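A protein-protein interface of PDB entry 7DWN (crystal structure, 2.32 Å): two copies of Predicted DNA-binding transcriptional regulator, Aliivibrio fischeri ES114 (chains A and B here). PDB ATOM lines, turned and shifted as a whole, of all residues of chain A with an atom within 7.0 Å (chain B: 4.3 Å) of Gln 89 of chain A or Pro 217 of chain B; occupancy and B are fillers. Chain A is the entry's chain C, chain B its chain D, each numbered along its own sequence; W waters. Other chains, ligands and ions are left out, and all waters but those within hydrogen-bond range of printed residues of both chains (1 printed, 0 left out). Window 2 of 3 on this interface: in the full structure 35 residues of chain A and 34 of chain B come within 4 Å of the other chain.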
ATOM      1  N   ILE A  84     -18.982  18.374   6.881  1.00  0.00           N
ATOM      2  CA  ILE A  84     -19.474  19.725   6.633  1.00  0.00           C
ATOM      3  C   ILE A  84     -19.419  20.603   7.870  1.00  0.00           C
ATOM      4  O   ILE A  84     -19.899  21.742   7.824  1.00  0.00           O
ATOM      5  CB  ILE A  84     -20.902  19.710   6.060  1.00  0.00           C
ATOM      6  CG1 ILE A  84     -21.908  19.263   7.126  1.00  0.00           C
ATOM      7  CG2 ILE A  84     -20.983  18.799   4.844  1.00  0.00           C
ATOM      8  CD1 ILE A  84     -23.352  19.397   6.704  1.00  0.00           C
ATOM      9  N   SER A  85     -18.849  20.114   8.975  1.00  0.00           N
ATOM     10  CA  SER A  85     -18.789  20.904  10.201  1.00  0.00           C
ATOM     11  C   SER A  85     -18.059  22.226   9.970  1.00  0.00           C
ATOM     12  O   SER A  85     -18.626  23.311  10.161  1.00  0.00           O
ATOM     13  CB  SER A  85     -18.111  20.082  11.304  1.00  0.00           C
ATOM     14  OG  SER A  85     -18.014  20.795  12.526  1.00  0.00           O
ATOM     15  N   ASP A  86     -16.791  22.145   9.554  1.00  0.00           N
ATOM     16  CA  ASP A  86     -15.996  23.342   9.295  1.00  0.00           C
ATOM     17  C   ASP A  86     -16.667  24.243   8.264  1.00  0.00           C
ATOM     18  O   ASP A  86     -16.793  25.456   8.468  1.00  0.00           O
ATOM     19  CB  ASP A  86     -14.596  22.941   8.823  1.00  0.00           C
ATOM     20  CG  ASP A  86     -13.849  22.109   9.849  1.00  0.00           C
ATOM     21  OD1 ASP A  86     -14.033  22.356  11.059  1.00  0.00           O
ATOM     22  OD2 ASP A  86     -13.075  21.213   9.446  1.00  0.00           O
ATOM     23  N   LEU A  87     -17.103  23.664   7.142  1.00  0.00           N
ATOM     24  CA  LEU A  87     -17.720  24.461   6.088  1.00  0.00           C
ATOM     25  C   LEU A  87     -18.992  25.141   6.576  1.00  0.00           C
ATOM     26  O   LEU A  87     -19.206  26.331   6.314  1.00  0.00           O
ATOM     27  CB  LEU A  87     -18.024  23.584   4.875  1.00  0.00           C
ATOM     28  CG  LEU A  87     -16.809  22.956   4.198  1.00  0.00           C
ATOM     29  CD1 LEU A  87     -17.231  22.194   2.956  1.00  0.00           C
ATOM     30  CD2 LEU A  87     -15.795  24.030   3.860  1.00  0.00           C
ATOM     31  N   SER A  88     -19.848  24.401   7.285  1.00  0.00           N
ATOM     32  CA  SER A  88     -21.096  24.980   7.771  1.00  0.00           C
ATOM     33  C   SER A  88     -20.847  26.102   8.766  1.00  0.00           C
ATOM     34  O   SER A  88     -21.620  27.067   8.814  1.00  0.00           O
ATOM     35  CB  SER A  88     -21.966  23.903   8.412  1.00  0.00           C
ATOM     36  OG  SER A  88     -21.403  23.445   9.627  1.00  0.00           O
ATOM     37  N   GLN A  89     -19.789  25.997   9.574  1.00  0.00           N
ATOM     38  CA  GLN A  89     -19.514  27.066  10.529  1.00  0.00           C
ATOM     39  C   GLN A  89     -19.241  28.390   9.821  1.00  0.00           C
ATOM     40  O   GLN A  89     -19.643  29.454  10.306  1.00  0.00           O
ATOM     41  CB  GLN A  89     -18.339  26.686  11.430  1.00  0.00           C
ATOM     42  CG  GLN A  89     -18.275  27.480  12.724  1.00  0.00           C
ATOM     43  CD  GLN A  89     -17.147  27.025  13.624  1.00  0.00           C
ATOM     44  OE1 GLN A  89     -16.072  26.657  13.150  1.00  0.00           O
ATOM     45  NE2 GLN A  89     -17.388  27.035  14.931  1.00  0.00           N
ATOM     46  N   LEU A  90     -18.582  28.346   8.661  1.00  0.00           N
ATOM     47  CA  LEU A  90     -18.171  29.565   7.973  1.00  0.00           C
ATOM     48  C   LEU A  90     -19.243  30.143   7.057  1.00  0.00           C
ATOM     49  O   LEU A  90     -19.190  31.338   6.745  1.00  0.00           O
ATOM     50  CB  LEU A  90     -16.895  29.311   7.163  1.00  0.00           C
ATOM     51  CG  LEU A  90     -15.668  28.926   7.995  1.00  0.00           C
ATOM     52  CD1 LEU A  90     -14.468  28.632   7.110  1.00  0.00           C
ATOM     53  CD2 LEU A  90     -15.339  30.020   9.000  1.00  0.00           C
ATOM     54  N   GLY A  91     -20.200  29.339   6.615  1.00  0.00           N
ATOM     55  CA  GLY A  91     -21.325  29.831   5.842  1.00  0.00           C
ATOM     56  C   GLY A  91     -21.234  29.438   4.377  1.00  0.00           C
ATOM     57  O   GLY A  91     -20.320  28.740   3.937  1.00  0.00           O
ATOM     58  N   VAL A  94     -18.032  30.117   1.967  1.00  0.00           N
ATOM     59  CA  VAL A  94     -16.752  29.533   2.350  1.00  0.00           C
ATOM     60  C   VAL A  94     -16.017  29.062   1.102  1.00  0.00           C
ATOM     61  O   VAL A  94     -16.610  28.481   0.186  1.00  0.00           O
ATOM     62  CB  VAL A  94     -16.950  28.386   3.360  1.00  0.00           C
ATOM     63  CG1 VAL A  94     -17.816  27.280   2.776  1.00  0.00           C
ATOM     64  CG2 VAL A  94     -15.604  27.829   3.798  1.00  0.00           C
ATOM     65  N   ILE A 123     -15.259  33.706   2.716  1.00  0.00           N
ATOM     66  CA  ILE A 123     -14.700  33.333   4.008  1.00  0.00           C
ATOM     67  C   ILE A 123     -13.723  32.196   3.755  1.00  0.00           C
ATOM     68  O   ILE A 123     -14.111  31.143   3.235  1.00  0.00           O
ATOM     69  CB  ILE A 123     -15.787  32.917   5.011  1.00  0.00           C
ATOM     70  CG1 ILE A 123     -16.812  34.039   5.187  1.00  0.00           C
ATOM     71  CG2 ILE A 123     -15.163  32.549   6.345  1.00  0.00           C
ATOM     72  CD1 ILE A 123     -16.226  35.319   5.742  1.00  0.00           C
ATOM     73  N   TRP B 193     -13.607  35.973  14.736  1.00  0.00           N
ATOM     74  CA  TRP B 193     -12.965  34.796  15.299  1.00  0.00           C
ATOM     75  C   TRP B 193     -12.206  34.074  14.196  1.00  0.00           C
ATOM     76  O   TRP B 193     -12.793  33.690  13.177  1.00  0.00           O
ATOM     77  CB  TRP B 193     -14.017  33.889  15.941  1.00  0.00           C
ATOM     78  CG  TRP B 193     -13.509  32.599  16.490  1.00  0.00           C
ATOM     79  CD1 TRP B 193     -12.255  32.335  16.957  1.00  0.00           C
ATOM     80  CD2 TRP B 193     -14.253  31.384  16.624  1.00  0.00           C
ATOM     81  NE1 TRP B 193     -12.174  31.028  17.376  1.00  0.00           N
ATOM     82  CE2 TRP B 193     -13.388  30.424  17.182  1.00  0.00           C
ATOM     83  CE3 TRP B 193     -15.569  31.017  16.325  1.00  0.00           C
ATOM     84  CZ2 TRP B 193     -13.795  29.120  17.446  1.00  0.00           C
ATOM     85  CZ3 TRP B 193     -15.971  29.724  16.589  1.00  0.00           C
ATOM     86  CH2 TRP B 193     -15.088  28.790  17.144  1.00  0.00           C
ATOM     87  N   THR B 195     -10.417  30.740  13.575  1.00  0.00           N
ATOM     88  CA  THR B 195     -10.571  29.454  14.235  1.00  0.00           C
ATOM     89  C   THR B 195      -9.749  28.372  13.546  1.00  0.00           C
ATOM     90  O   THR B 195      -9.309  28.520  12.402  1.00  0.00           O
ATOM     91  CB  THR B 195     -12.045  29.025  14.271  1.00  0.00           C
ATOM     92  OG1 THR B 195     -12.176  27.823  15.038  1.00  0.00           O
ATOM     93  CG2 THR B 195     -12.562  28.775  12.861  1.00  0.00           C
ATOM     94  N   SER B 198     -12.516  22.338  13.122  1.00  0.00           N
ATOM     95  CA  SER B 198     -13.226  21.795  14.275  1.00  0.00           C
ATOM     96  C   SER B 198     -12.839  20.353  14.570  1.00  0.00           C
ATOM     97  O   SER B 198     -13.022  19.894  15.702  1.00  0.00           O
ATOM     98  CB  SER B 198     -14.737  21.890  14.060  1.00  0.00           C
ATOM     99  OG  SER B 198     -15.123  23.213  13.731  1.00  0.00           O
ATOM    100  N   LEU B 215     -18.802  34.684  19.525  1.00  0.00           N
ATOM    101  CA  LEU B 215     -17.791  34.618  18.480  1.00  0.00           C
ATOM    102  C   LEU B 215     -18.467  34.501  17.122  1.00  0.00           C
ATOM    103  O   LEU B 215     -19.491  33.825  16.991  1.00  0.00           O
ATOM    104  CB  LEU B 215     -16.856  33.421  18.689  1.00  0.00           C
ATOM    105  CG  LEU B 215     -16.127  33.316  20.030  1.00  0.00           C
ATOM    106  CD1 LEU B 215     -15.456  31.958  20.162  1.00  0.00           C
ATOM    107  CD2 LEU B 215     -15.108  34.431  20.167  1.00  0.00           C
ATOM    108  N   THR B 216     -17.895  35.152  16.115  1.00  0.00           N
ATOM    109  CA  THR B 216     -18.343  34.962  14.738  1.00  0.00           C
ATOM    110  C   THR B 216     -17.169  34.482  13.901  1.00  0.00           C
ATOM    111  O   THR B 216     -16.196  35.237  13.713  1.00  0.00           O
ATOM    112  CB  THR B 216     -18.925  36.251  14.152  1.00  0.00           C
ATOM    113  OG1 THR B 216     -18.151  37.373  14.593  1.00  0.00           O
ATOM    114  CG2 THR B 216     -20.373  36.425  14.588  1.00  0.00           C
ATOM    115  N   PRO B 217     -17.196  33.248  13.394  1.00  0.00           N
ATOM    116  CA  PRO B 217     -16.040  32.717  12.656  1.00  0.00           C
ATOM    117  C   PRO B 217     -15.926  33.366  11.286  1.00  0.00           C
ATOM    118  O   PRO B 217     -16.827  33.251  10.452  1.00  0.00           O
ATOM    119  CB  PRO B 217     -16.348  31.220  12.550  1.00  0.00           C
ATOM    120  CG  PRO B 217     -17.841  31.148  12.596  1.00  0.00           C
ATOM    121  CD  PRO B 217     -18.289  32.264  13.503  1.00  0.00           C
ATOM    122  N   ILE B 218     -14.806  34.050  11.051  1.00  0.00           N
ATOM    123  CA  ILE B 218     -14.571  34.723   9.778  1.00  0.00           C
ATOM    124  C   ILE B 218     -13.433  34.103   8.993  1.00  0.00           C
ATOM    125  O   ILE B 218     -13.122  34.582   7.892  1.00  0.00           O
ATOM    126  CB  ILE B 218     -14.316  36.229   9.974  1.00  0.00           C
ATOM    127  CG1 ILE B 218     -12.981  36.450  10.689  1.00  0.00           C
ATOM    128  CG2 ILE B 218     -15.466  36.867  10.742  1.00  0.00           C
ATOM    129  CD1 ILE B 218     -12.378  37.817  10.451  1.00  0.00           C
ATOM    130  N   PHE B 219     -12.803  33.052   9.513  1.00  0.00           N
ATOM    131  CA  PHE B 219     -11.615  32.482   8.895  1.00  0.00           C
ATOM    132  C   PHE B 219     -11.263  31.189   9.611  1.00  0.00           C
ATOM    133  O   PHE B 219     -11.381  31.108  10.836  1.00  0.00           O
ATOM    134  CB  PHE B 219     -10.443  33.467   8.965  1.00  0.00           C
ATOM    135  CG  PHE B 219      -9.185  32.959   8.340  1.00  0.00           C
ATOM    136  CD1 PHE B 219      -8.941  33.159   6.993  1.00  0.00           C
ATOM    137  CD2 PHE B 219      -8.242  32.288   9.100  1.00  0.00           C
ATOM    138  CE1 PHE B 219      -7.782  32.697   6.413  1.00  0.00           C
ATOM    139  CE2 PHE B 219      -7.082  31.826   8.527  1.00  0.00           C
ATOM    140  CZ  PHE B 219      -6.852  32.033   7.182  1.00  0.00           C
HETATM  141  O   HOH W   1     -14.362  25.944  14.957  1.00  0.00           O
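Pro 217 of chain B touches just these residues of chain A: Gln 89 (3.4 Å) and Leu 90 (3.8 Å). Of the printed residues of chain A, Ser 198 of chain B touches Ser 85 (3.8 Å), Asp 86 (2.6 Å) and Gln 89 (3.6 Å). Printed residues of chain B within 4 Å of Ser 85 of chain A: Ser 198. Leu 215 of chain B touches none of the printed residues of chain A. The nearest printed residue of chain B that does not touch Asp 86 of chain A is Thr 195 of chain B (6.8 Å).
The side-chain carboxylate of Asp 86 of chain A is in hydrogen-bond range of the backbone NH of Ser 198 of chain B (2.6 Å).
The backbone carbonyl oxygen (O) of Trp 193 of chain B lies within hydrogen-bond range of the backbone NH (N) of Ile 218 of chain B. The side-chain hydroxyl (OG) of Ser 88 of chain A is in hydrogen-bond range of the backbone carbonyl oxygen (O) of Ser 85 of chain A (2.8 Å). O of Phe 219 of chain B is in hydrogen-bond range of N of Thr 195 of chain B (2.9 Å). N of Trp 193 of chain B is in hydrogen-bond range of O of Thr 216 of chain B (2.9 Å).
Water W1 lies within hydrogen-bond range of OE1 of Gln 89 of chain A, OG1 of Thr 195 of chain B and OG of Ser 198 of chain B.
No position is printed for both chains. Of the 9 pairs that touch across the chains among the printed residues, none has its exchanged pair printed and touching as well.
Hydrophobic or aromatic side chains of chain B within 4 Å of the printed part of chain A: Trp 193 and Pro 217. Hydrophobic or aromatic side chains of chain A within 4 Å of the printed part of chain B: Leu 90 and Ile 123. Among the printed residues, no Asp or Glu carboxylate lies within 4 Å of a Lys or Arg side-chain nitrogen of the other chain.
Among the printed residues, merely in contact across the chains: Ile 123 of chain A with Ile 218 of chain B, Gln 89 of chain A with Pro 217 of chain B, Gln 89 of chain A with Trp 193 of chain B, Gln 89 of chain A with Ser 198 of chain B, Ser 85 of chain A with Ser 198 of chain B, Leu 90 of chain A with Pro 217 of chain B, Ile 123 of chain A with Phe 219 of chain B and Leu 90 of chain A with Phe 219 of chain B.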
